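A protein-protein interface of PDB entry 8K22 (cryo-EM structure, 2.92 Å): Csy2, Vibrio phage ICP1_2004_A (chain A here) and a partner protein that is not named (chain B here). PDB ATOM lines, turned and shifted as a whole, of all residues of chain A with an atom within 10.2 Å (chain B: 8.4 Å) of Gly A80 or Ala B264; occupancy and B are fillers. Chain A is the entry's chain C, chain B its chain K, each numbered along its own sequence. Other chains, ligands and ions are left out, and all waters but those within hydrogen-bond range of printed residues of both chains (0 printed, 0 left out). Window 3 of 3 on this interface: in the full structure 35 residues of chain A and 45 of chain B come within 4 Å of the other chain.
Among the printed residues, pairs that only touch across the chains: Ala A82 with Ser B254 (3.3 Å), Asn A83 with Gly B259 (3.3 Å), Trp A73 with Pro B251 (3.5 Å), Arg A76 with Tyr B252 (3.5 Å), Trp A73 with Tyr B252 (3.5 Å), Gly A79 with Tyr B252 (3.5 Å), Asn A83 with Ala B261 (3.7 Å), Ala A82 with Tyr B252 (3.7 Å), Ala A82 with Ala B261 (3.8 Å), Asn A83 with Val B260 (3.9 Å) and Gly A80 with Ala B264 (3.9 Å).
Printed residues of chain B within 4 Å of Asp A75: Tyr B252 (2.8 Å). Of the printed residues of chain B, Gly A77 touches Tyr B252 (2.9 Å). Of chain B, only Tyr B252 (3.5 Å) comes within 4 Å of Gly A79. Gly A80 touches just one residue of chain B: Ala B264. Asn A84 touches none of the printed residues of chain B. Asn A85 touches none of the printed residues of chain B. Of the printed residues of chain A, Pro B251 touches Trp A73 (3.5 Å). No residue of chain A comes within 4 Å of Gly B253. Of the printed residues of chain A, Val B260 touches Asn A83. Of chain A, only Ala A82 and Asn A83 come within 4 Å of Ala B261. Ala B264 touches just one residue of chain A: Gly A80 (3.9 Å). The nearest residue of chain B that does not touch Gly A80 is Gly B265 (5.4 Å). The nearest printed residue of chain A that does not touch Val B260 is Ala A82 (5.3 Å).
Of the 21 printed residues of chain B, 7 touch a printed residue of chain A. Hydrophobic or aromatic side chains of chain B within 4 Å of the printed part of chain A: Pro B251, Tyr B252, Ala B261 and Ala B264. Hydrophobic or aromatic side chains of chain A within 4 Å of the printed part of chain B: Trp A73 and Ala A82. Among the printed residues, 14 pairs touch across the chains. Among the printed residues, no Asp or Glu carboxylate lies within 4 Å of a Lys or Arg side-chain nitrogen of the other chain.
O of Asp A75 sits at hydrogen-bond distance from OH of Tyr B252 (2.8 Å). The backbone NH (N) of Gly A77 sits at hydrogen-bond distance from the side-chain hydroxyl (OH) of Tyr B252, at 2.9 Å. The side-chain amide oxygen (OD1) of Asn A78 lies within hydrogen-bond range of the side-chain hydroxyl (OH) of Tyr B252.
The side-chain amide oxygen (OD1) of Asn B266 sits close to the backbone carbonyl oxygen (O) of Ala B264, 3.4 Å away. The backbone carbonyl oxygen of Tyr B252 is in hydrogen-bond range of the backbone NH of Arg B263. The indole nitrogen (NE1) of Trp A73 is in hydrogen-bond range of the backbone carbonyl oxygen (O) of Asn A84 (2.7 Å). The backbone carbonyl oxygen (O) of Lys A81 sits close to the indole nitrogen (NE1) of Trp A73 (3.3 Å). The backbone carbonyl oxygen (O) of Tyr B252 lies within hydrogen-bond range of the backbone NH (N) of Ala B264 (3.5 Å). The side-chain amide oxygen of Asn A78 sits close to the backbone carbonyl oxygen of Asp A75 (2.9 Å).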
ATOM      1  N   TRP A  73     -16.745  30.246  20.552  1.00  0.00           N
ATOM      2  CA  TRP A  73     -15.704  29.255  20.323  1.00  0.00           C
ATOM      3  C   TRP A  73     -16.322  27.870  20.223  1.00  0.00           C
ATOM      4  O   TRP A  73     -16.517  27.194  21.237  1.00  0.00           O
ATOM      5  CB  TRP A  73     -14.664  29.303  21.440  1.00  0.00           C
ATOM      6  CG  TRP A  73     -13.674  30.401  21.278  1.00  0.00           C
ATOM      7  CD1 TRP A  73     -13.614  31.557  21.991  1.00  0.00           C
ATOM      8  CD2 TRP A  73     -12.594  30.448  20.343  1.00  0.00           C
ATOM      9  NE1 TRP A  73     -12.560  32.321  21.563  1.00  0.00           N
ATOM     10  CE2 TRP A  73     -11.918  31.661  20.549  1.00  0.00           C
ATOM     11  CE3 TRP A  73     -12.134  29.580  19.351  1.00  0.00           C
ATOM     12  CZ2 TRP A  73     -10.809  32.034  19.798  1.00  0.00           C
ATOM     13  CZ3 TRP A  73     -11.031  29.951  18.609  1.00  0.00           C
ATOM     14  CH2 TRP A  73     -10.381  31.166  18.837  1.00  0.00           C
ATOM     15  N   ASP A  75     -15.375  25.597  17.368  1.00  0.00           N
ATOM     16  CA  ASP A  75     -14.549  24.643  16.652  1.00  0.00           C
ATOM     17  C   ASP A  75     -13.786  23.765  17.638  1.00  0.00           C
ATOM     18  O   ASP A  75     -13.667  24.078  18.824  1.00  0.00           O
ATOM     19  CB  ASP A  75     -13.581  25.361  15.715  1.00  0.00           C
ATOM     20  CG  ASP A  75     -14.254  25.855  14.454  1.00  0.00           C
ATOM     21  OD1 ASP A  75     -15.405  25.445  14.194  1.00  0.00           O
ATOM     22  OD2 ASP A  75     -13.634  26.654  13.720  1.00  0.00           O
ATOM     23  N   ARG A  76     -13.272  22.652  17.136  1.00  0.00           N
ATOM     24  CA  ARG A  76     -12.579  21.673  17.959  1.00  0.00           C
ATOM     25  C   ARG A  76     -11.076  21.877  17.855  1.00  0.00           C
ATOM     26  O   ARG A  76     -10.537  22.064  16.762  1.00  0.00           O
ATOM     27  CB  ARG A  76     -12.947  20.251  17.531  1.00  0.00           C
ATOM     28  CG  ARG A  76     -12.297  19.147  18.349  1.00  0.00           C
ATOM     29  CD  ARG A  76     -12.633  17.778  17.784  1.00  0.00           C
ATOM     30  NE  ARG A  76     -13.948  17.773  17.155  1.00  0.00           N
ATOM     31  CZ  ARG A  76     -15.027  17.219  17.686  1.00  0.00           C
ATOM     32  NH1 ARG A  76     -14.980  16.580  18.841  1.00  0.00           N
ATOM     33  NH2 ARG A  76     -16.185  17.306  17.036  1.00  0.00           N
ATOM     34  N   GLY A  77     -10.404  21.849  19.000  1.00  0.00           N
ATOM     35  CA  GLY A  77      -8.962  21.893  19.045  1.00  0.00           C
ATOM     36  C   GLY A  77      -8.368  23.245  19.365  1.00  0.00           C
ATOM     37  O   GLY A  77      -7.152  23.333  19.568  1.00  0.00           O
ATOM     38  N   ASN A  78      -9.178  24.302  19.416  1.00  0.00           N
ATOM     39  CA  ASN A  78      -8.684  25.627  19.766  1.00  0.00           C
ATOM     40  C   ASN A  78      -9.012  26.004  21.205  1.00  0.00           C
ATOM     41  O   ASN A  78      -9.287  27.172  21.494  1.00  0.00           O
ATOM     42  CB  ASN A  78      -9.220  26.680  18.799  1.00  0.00           C
ATOM     43  CG  ASN A  78     -10.667  26.467  18.448  1.00  0.00           C
ATOM     44  OD1 ASN A  78     -11.422  25.871  19.210  1.00  0.00           O
ATOM     45  ND2 ASN A  78     -11.064  26.951  17.280  1.00  0.00           N
ATOM     46  N   GLY A  79      -9.010  25.030  22.111  1.00  0.00           N
ATOM     47  CA  GLY A  79      -9.023  25.347  23.522  1.00  0.00           C
ATOM     48  C   GLY A  79      -7.718  25.990  23.946  1.00  0.00           C
ATOM     49  O   GLY A  79      -6.658  25.741  23.377  1.00  0.00           O
ATOM     50  N   GLY A  80      -7.802  26.846  24.955  1.00  0.00           N
ATOM     51  CA  GLY A  80      -6.651  27.640  25.333  1.00  0.00           C
ATOM     52  C   GLY A  80      -6.744  29.024  24.734  1.00  0.00           C
ATOM     53  O   GLY A  80      -6.391  30.018  25.376  1.00  0.00           O
ATOM     54  N   LYS A  81      -7.216  29.097  23.494  1.00  0.00           N
ATOM     55  CA  LYS A  81      -7.599  30.356  22.874  1.00  0.00           C
ATOM     56  C   LYS A  81      -9.047  30.722  23.160  1.00  0.00           C
ATOM     57  O   LYS A  81      -9.501  31.781  22.717  1.00  0.00           O
ATOM     58  CB  LYS A  81      -7.379  30.296  21.362  1.00  0.00           C
ATOM     59  CG  LYS A  81      -6.056  29.684  20.949  1.00  0.00           C
ATOM     60  CD  LYS A  81      -5.749  29.963  19.488  1.00  0.00           C
ATOM     61  CE  LYS A  81      -6.881  29.516  18.586  1.00  0.00           C
ATOM     62  NZ  LYS A  81      -6.539  29.678  17.148  1.00  0.00           N
ATOM     63  N   ALA A  82      -9.775  29.875  23.886  1.00  0.00           N
ATOM     64  CA  ALA A  82     -11.192  30.110  24.125  1.00  0.00           C
ATOM     65  C   ALA A  82     -11.447  31.238  25.111  1.00  0.00           C
ATOM     66  O   ALA A  82     -12.542  31.807  25.103  1.00  0.00           O
ATOM     67  CB  ALA A  82     -11.855  28.832  24.630  1.00  0.00           C
ATOM     68  N   ASN A  83     -10.472  31.568  25.964  1.00  0.00           N
ATOM     69  CA  ASN A  83     -10.647  32.679  26.891  1.00  0.00           C
ATOM     70  C   ASN A  83     -10.717  34.015  26.165  1.00  0.00           C
ATOM     71  O   ASN A  83     -11.498  34.889  26.557  1.00  0.00           O
ATOM     72  CB  ASN A  83      -9.519  32.689  27.920  1.00  0.00           C
ATOM     73  CG  ASN A  83      -8.198  32.261  27.335  1.00  0.00           C
ATOM     74  OD1 ASN A  83      -7.973  32.376  26.132  1.00  0.00           O
ATOM     75  ND2 ASN A  83      -7.309  31.764  28.184  1.00  0.00           N
ATOM     76  N   ASN A  84      -9.933  34.187  25.107  1.00  0.00           N
ATOM     77  CA  ASN A  84     -10.016  35.390  24.296  1.00  0.00           C
ATOM     78  C   ASN A  84     -11.265  35.363  23.422  1.00  0.00           C
ATOM     79  O   ASN A  84     -11.957  34.348  23.307  1.00  0.00           O
ATOM     80  CB  ASN A  84      -8.769  35.547  23.431  1.00  0.00           C
ATOM     81  CG  ASN A  84      -7.503  35.160  24.160  1.00  0.00           C
ATOM     82  OD1 ASN A  84      -7.466  35.134  25.388  1.00  0.00           O
ATOM     83  ND2 ASN A  84      -6.454  34.855  23.405  1.00  0.00           N
ATOM     84  N   ASN A  85     -11.552  36.508  22.810  1.00  0.00           N
ATOM     85  CA  ASN A  85     -12.719  36.642  21.953  1.00  0.00           C
ATOM     86  C   ASN A  85     -12.551  35.823  20.682  1.00  0.00           C
ATOM     87  O   ASN A  85     -11.464  35.763  20.101  1.00  0.00           O
ATOM     88  CB  ASN A  85     -12.950  38.107  21.600  1.00  0.00           C
ATOM     89  CG  ASN A  85     -13.485  38.902  22.763  1.00  0.00           C
ATOM     90  OD1 ASN A  85     -12.776  39.154  23.735  1.00  0.00           O
ATOM     91  ND2 ASN A  85     -14.745  39.309  22.671  1.00  0.00           N
ATOM     92  N   TYR B 240     -18.988  23.210  35.828  1.00  0.00           N
ATOM     93  CA  TYR B 240     -17.586  23.272  35.462  1.00  0.00           C
ATOM     94  C   TYR B 240     -16.715  23.156  36.712  1.00  0.00           C
ATOM     95  O   TYR B 240     -17.207  23.033  37.838  1.00  0.00           O
ATOM     96  CB  TYR B 240     -17.303  24.550  34.674  1.00  0.00           C
ATOM     97  CG  TYR B 240     -17.753  25.832  35.343  1.00  0.00           C
ATOM     98  CD1 TYR B 240     -16.911  26.525  36.200  1.00  0.00           C
ATOM     99  CD2 TYR B 240     -19.016  26.357  35.106  1.00  0.00           C
ATOM    100  CE1 TYR B 240     -17.315  27.695  36.802  1.00  0.00           C
ATOM    101  CE2 TYR B 240     -19.426  27.522  35.709  1.00  0.00           C
ATOM    102  CZ  TYR B 240     -18.574  28.185  36.556  1.00  0.00           C
ATOM    103  OH  TYR B 240     -18.981  29.350  37.157  1.00  0.00           O
ATOM    104  N   GLU B 241     -15.401  23.180  36.514  1.00  0.00           N
ATOM    105  CA  GLU B 241     -14.475  23.062  37.632  1.00  0.00           C
ATOM    106  C   GLU B 241     -14.463  24.347  38.451  1.00  0.00           C
ATOM    107  O   GLU B 241     -14.344  25.442  37.893  1.00  0.00           O
ATOM    108  CB  GLU B 241     -13.071  22.743  37.125  1.00  0.00           C
ATOM    109  CG  GLU B 241     -12.795  21.260  36.985  1.00  0.00           C
ATOM    110  CD  GLU B 241     -12.621  20.578  38.324  1.00  0.00           C
ATOM    111  OE1 GLU B 241     -13.130  19.449  38.492  1.00  0.00           O
ATOM    112  OE2 GLU B 241     -11.973  21.171  39.212  1.00  0.00           O
ATOM    113  N   ILE B 247     -22.651  29.880  34.112  1.00  0.00           N
ATOM    114  CA  ILE B 247     -22.150  30.470  32.884  1.00  0.00           C
ATOM    115  C   ILE B 247     -22.953  29.899  31.721  1.00  0.00           C
ATOM    116  O   ILE B 247     -23.721  28.951  31.873  1.00  0.00           O
ATOM    117  CB  ILE B 247     -20.644  30.229  32.692  1.00  0.00           C
ATOM    118  CG1 ILE B 247     -20.384  28.757  32.388  1.00  0.00           C
ATOM    119  CG2 ILE B 247     -19.876  30.668  33.924  1.00  0.00           C
ATOM    120  CD1 ILE B 247     -18.953  28.447  32.072  1.00  0.00           C
ATOM    121  N   PRO B 251     -19.129  25.349  24.049  1.00  0.00           N
ATOM    122  CA  PRO B 251     -18.302  24.147  23.865  1.00  0.00           C
ATOM    123  C   PRO B 251     -17.069  24.105  24.750  1.00  0.00           C
ATOM    124  O   PRO B 251     -16.641  23.013  25.142  1.00  0.00           O
ATOM    125  CB  PRO B 251     -17.935  24.211  22.381  1.00  0.00           C
ATOM    126  CG  PRO B 251     -19.083  24.905  21.770  1.00  0.00           C
ATOM    127  CD  PRO B 251     -19.481  25.958  22.757  1.00  0.00           C
ATOM    128  N   TYR B 252     -16.489  25.254  25.086  1.00  0.00           N
ATOM    129  CA  TYR B 252     -15.353  25.313  25.994  1.00  0.00           C
ATOM    130  C   TYR B 252     -15.687  25.980  27.318  1.00  0.00           C
ATOM    131  O   TYR B 252     -14.769  26.269  28.092  1.00  0.00           O
ATOM    132  CB  TYR B 252     -14.184  26.047  25.343  1.00  0.00           C
ATOM    133  CG  TYR B 252     -13.578  25.337  24.166  1.00  0.00           C
ATOM    134  CD1 TYR B 252     -12.841  24.175  24.339  1.00  0.00           C
ATOM    135  CD2 TYR B 252     -13.732  25.834  22.884  1.00  0.00           C
ATOM    136  CE1 TYR B 252     -12.280  23.525  23.265  1.00  0.00           C
ATOM    137  CE2 TYR B 252     -13.177  25.192  21.805  1.00  0.00           C
ATOM    138  CZ  TYR B 252     -12.448  24.040  22.001  1.00  0.00           C
ATOM    139  OH  TYR B 252     -11.893  23.395  20.922  1.00  0.00           O
ATOM    140  N   GLY B 253     -16.964  26.235  27.592  1.00  0.00           N
ATOM    141  CA  GLY B 253     -17.369  26.945  28.800  1.00  0.00           C
ATOM    142  C   GLY B 253     -16.802  28.344  28.877  1.00  0.00           C
ATOM    143  O   GLY B 253     -16.423  28.805  29.959  1.00  0.00           O
ATOM    144  N   SER B 254     -16.720  29.023  27.743  1.00  0.00           N
ATOM    145  CA  SER B 254     -15.887  30.206  27.599  1.00  0.00           C
ATOM    146  C   SER B 254     -16.747  31.456  27.602  1.00  0.00           C
ATOM    147  O   SER B 254     -17.537  31.671  26.678  1.00  0.00           O
ATOM    148  CB  SER B 254     -15.081  30.127  26.307  1.00  0.00           C
ATOM    149  OG  SER B 254     -15.931  30.196  25.177  1.00  0.00           O
ATOM    150  N   GLY B 259     -13.141  37.080  29.700  1.00  0.00           N
ATOM    151  CA  GLY B 259     -11.804  36.655  29.347  1.00  0.00           C
ATOM    152  C   GLY B 259     -11.349  35.367  29.991  1.00  0.00           C
ATOM    153  O   GLY B 259     -10.144  35.144  30.117  1.00  0.00           O
ATOM    154  N   VAL B 260     -12.276  34.512  30.407  1.00  0.00           N
ATOM    155  CA  VAL B 260     -11.946  33.262  31.078  1.00  0.00           C
ATOM    156  C   VAL B 260     -12.770  32.133  30.470  1.00  0.00           C
ATOM    157  O   VAL B 260     -13.964  32.295  30.193  1.00  0.00           O
ATOM    158  CB  VAL B 260     -12.147  33.385  32.611  1.00  0.00           C
ATOM    159  CG1 VAL B 260     -13.542  33.882  32.964  1.00  0.00           C
ATOM    160  CG2 VAL B 260     -11.836  32.075  33.330  1.00  0.00           C
ATOM    161  N   ALA B 261     -12.112  31.008  30.197  1.00  0.00           N
ATOM    162  CA  ALA B 261     -12.757  29.802  29.686  1.00  0.00           C
ATOM    163  C   ALA B 261     -12.658  28.730  30.760  1.00  0.00           C
ATOM    164  O   ALA B 261     -11.573  28.196  31.009  1.00  0.00           O
ATOM    165  CB  ALA B 261     -12.105  29.341  28.387  1.00  0.00           C
ATOM    166  N   TYR B 262     -13.785  28.414  31.396  1.00  0.00           N
ATOM    167  CA  TYR B 262     -13.746  27.543  32.563  1.00  0.00           C
ATOM    168  C   TYR B 262     -13.628  26.067  32.221  1.00  0.00           C
ATOM    169  O   TYR B 262     -13.247  25.280  33.092  1.00  0.00           O
ATOM    170  CB  TYR B 262     -14.977  27.733  33.451  1.00  0.00           C
ATOM    171  CG  TYR B 262     -15.231  29.137  33.953  1.00  0.00           C
ATOM    172  CD1 TYR B 262     -15.847  30.094  33.159  1.00  0.00           C
ATOM    173  CD2 TYR B 262     -14.823  29.510  35.227  1.00  0.00           C
ATOM    174  CE1 TYR B 262     -16.074  31.365  33.631  1.00  0.00           C
ATOM    175  CE2 TYR B 262     -15.044  30.780  35.703  1.00  0.00           C
ATOM    176  CZ  TYR B 262     -15.666  31.705  34.900  1.00  0.00           C
ATOM    177  OH  TYR B 262     -15.886  32.979  35.369  1.00  0.00           O
ATOM    178  N   ARG B 263     -13.942  25.664  30.992  1.00  0.00           N
ATOM    179  CA  ARG B 263     -13.888  24.255  30.629  1.00  0.00           C
ATOM    180  C   ARG B 263     -12.812  23.971  29.591  1.00  0.00           C
ATOM    181  O   ARG B 263     -12.840  22.920  28.949  1.00  0.00           O
ATOM    182  CB  ARG B 263     -15.248  23.778  30.125  1.00  0.00           C
ATOM    183  CG  ARG B 263     -16.249  23.516  31.223  1.00  0.00           C
ATOM    184  CD  ARG B 263     -17.630  23.363  30.646  1.00  0.00           C
ATOM    185  NE  ARG B 263     -18.628  23.073  31.666  1.00  0.00           N
ATOM    186  CZ  ARG B 263     -19.051  21.854  31.966  1.00  0.00           C
ATOM    187  NH1 ARG B 263     -18.554  20.784  31.369  1.00  0.00           N
ATOM    188  NH2 ARG B 263     -19.992  21.704  32.893  1.00  0.00           N
ATOM    189  N   ALA B 264     -11.854  24.874  29.423  1.00  0.00           N
ATOM    190  CA  ALA B 264     -10.781  24.704  28.455  1.00  0.00           C
ATOM    191  C   ALA B 264      -9.515  24.257  29.169  1.00  0.00           C
ATOM    192  O   ALA B 264      -9.061  24.917  30.108  1.00  0.00           O
ATOM    193  CB  ALA B 264     -10.523  26.000  27.687  1.00  0.00           C
ATOM    194  N   GLY B 265      -8.952  23.138  28.721  1.00  0.00           N
ATOM    195  CA  GLY B 265      -7.686  22.658  29.218  1.00  0.00           C
ATOM    196  C   GLY B 265      -7.761  21.690  30.377  1.00  0.00           C
ATOM    197  O   GLY B 265      -6.743  21.069  30.705  1.00  0.00           O
ATOM    198  N   ASN B 266      -8.922  21.534  31.007  1.00  0.00           N
ATOM    199  CA  ASN B 266      -9.071  20.617  32.128  1.00  0.00           C
ATOM    200  C   ASN B 266      -9.932  19.414  31.773  1.00  0.00           C
ATOM    201  O   ASN B 266     -10.528  18.801  32.668  1.00  0.00           O
ATOM    202  CB  ASN B 266      -9.635  21.348  33.345  1.00  0.00           C
ATOM    203  CG  ASN B 266     -10.762  22.278  32.990  1.00  0.00           C
ATOM    204  OD1 ASN B 266     -10.899  22.694  31.842  1.00  0.00           O
ATOM    205  ND2 ASN B 266     -11.579  22.618  33.977  1.00  0.00           N
ATOM    206  N   LYS B 267     -10.000  19.081  30.477  1.00  0.00           N
ATOM    207  CA  LYS B 267     -10.622  17.861  29.945  1.00  0.00           C
ATOM    208  C   LYS B 267     -12.101  17.767  30.307  1.00  0.00           C
ATOM    209  O   LYS B 267     -12.624  16.684  30.579  1.00  0.00           O
ATOM    210  CB  LYS B 267      -9.870  16.607  30.395  1.00  0.00           C
ATOM    211  CG  LYS B 267      -8.656  16.270  29.533  1.00  0.00           C
ATOM    212  CD  LYS B 267      -7.712  15.174  30.092  1.00  0.00           C
ATOM    213  CE  LYS B 267      -8.325  13.963  30.847  1.00  0.00           C
ATOM    214  NZ  LYS B 267      -9.642  13.381  30.418  1.00  0.00           N
ATOM    215  N   THR B 268     -12.779  18.912  30.322  1.00  0.00           N
ATOM    216  CA  THR B 268     -14.208  18.948  30.596  1.00  0.00           C
ATOM    217  C   THR B 268     -14.951  19.811  29.586  1.00  0.00           C
ATOM    218  O   THR B 268     -16.070  20.257  29.860  1.00  0.00           O
ATOM    219  CB  THR B 268     -14.486  19.438  32.020  1.00  0.00           C
ATOM    220  OG1 THR B 268     -15.899  19.531  32.226  1.00  0.00           O
ATOM    221  CG2 THR B 268     -13.864  20.795  32.247  1.00  0.00           C
ATOM    222  N   ASP B 269     -14.362  20.047  28.416  1.00  0.00           N
ATOM    223  CA  ASP B 269     -15.061  20.758  27.359  1.00  0.00           C
ATOM    224  C   ASP B 269     -16.062  19.829  26.677  1.00  0.00           C
ATOM    225  O   ASP B 269     -16.235  18.669  27.057  1.00  0.00           O
ATOM    226  CB  ASP B 269     -14.068  21.348  26.360  1.00  0.00           C
ATOM    227  CG  ASP B 269     -12.946  20.396  26.008  1.00  0.00           C
ATOM    228  OD1 ASP B 269     -13.221  19.233  25.661  1.00  0.00           O
ATOM    229  OD2 ASP B 269     -11.775  20.818  26.081  1.00  0.00           O
ATOM    230  N   LEU B 270     -16.733  20.347  25.649  1.00  0.00           N
ATOM    231  CA  LEU B 270     -17.751  19.558  24.966  1.00  0.00           C
ATOM    232  C   LEU B 270     -17.130  18.427  24.159  1.00  0.00           C
ATOM    233  O   LEU B 270     -17.698  17.335  24.081  1.00  0.00           O
ATOM    234  CB  LEU B 270     -18.600  20.460  24.074  1.00  0.00           C
ATOM    235  CG  LEU B 270     -19.365  19.870  22.889  1.00  0.00           C
ATOM    236  CD1 LEU B 270     -20.498  18.966  23.353  1.00  0.00           C
ATOM    237  CD2 LEU B 270     -19.889  20.979  22.012  1.00  0.00           C
ATOM    238  N   THR B 272     -14.147  16.665  24.500  1.00  0.00           N
ATOM    239  CA  THR B 272     -13.612  15.536  25.255  1.00  0.00           C
ATOM    240  C   THR B 272     -14.727  14.684  25.846  1.00  0.00           C
ATOM    241  O   THR B 272     -14.682  13.451  25.767  1.00  0.00           O
ATOM    242  CB  THR B 272     -12.679  16.033  26.357  1.00  0.00           C
ATOM    243  OG1 THR B 272     -11.753  16.976  25.804  1.00  0.00           O
ATOM    244  CG2 THR B 272     -11.908  14.876  26.964  1.00  0.00           C
ATOM    245  N   PHE B 290     -24.411  18.546  30.236  1.00  0.00           N
ATOM    246  CA  PHE B 290     -23.656  19.596  29.556  1.00  0.00           C
ATOM    247  C   PHE B 290     -23.564  19.343  28.053  1.00  0.00           C
ATOM    248  O   PHE B 290     -23.743  20.267  27.247  1.00  0.00           O
ATOM    249  CB  PHE B 290     -22.262  19.707  30.169  1.00  0.00           C
ATOM    250  CG  PHE B 290     -21.320  20.562  29.381  1.00  0.00           C
ATOM    251  CD1 PHE B 290     -21.467  21.938  29.359  1.00  0.00           C
ATOM    252  CD2 PHE B 290     -20.280  19.990  28.670  1.00  0.00           C
ATOM    253  CE1 PHE B 290     -20.596  22.725  28.640  1.00  0.00           C
ATOM    254  CE2 PHE B 290     -19.410  20.772  27.948  1.00  0.00           C
ATOM    255  CZ  PHE B 290     -19.569  22.136  27.930  1.00  0.00           C
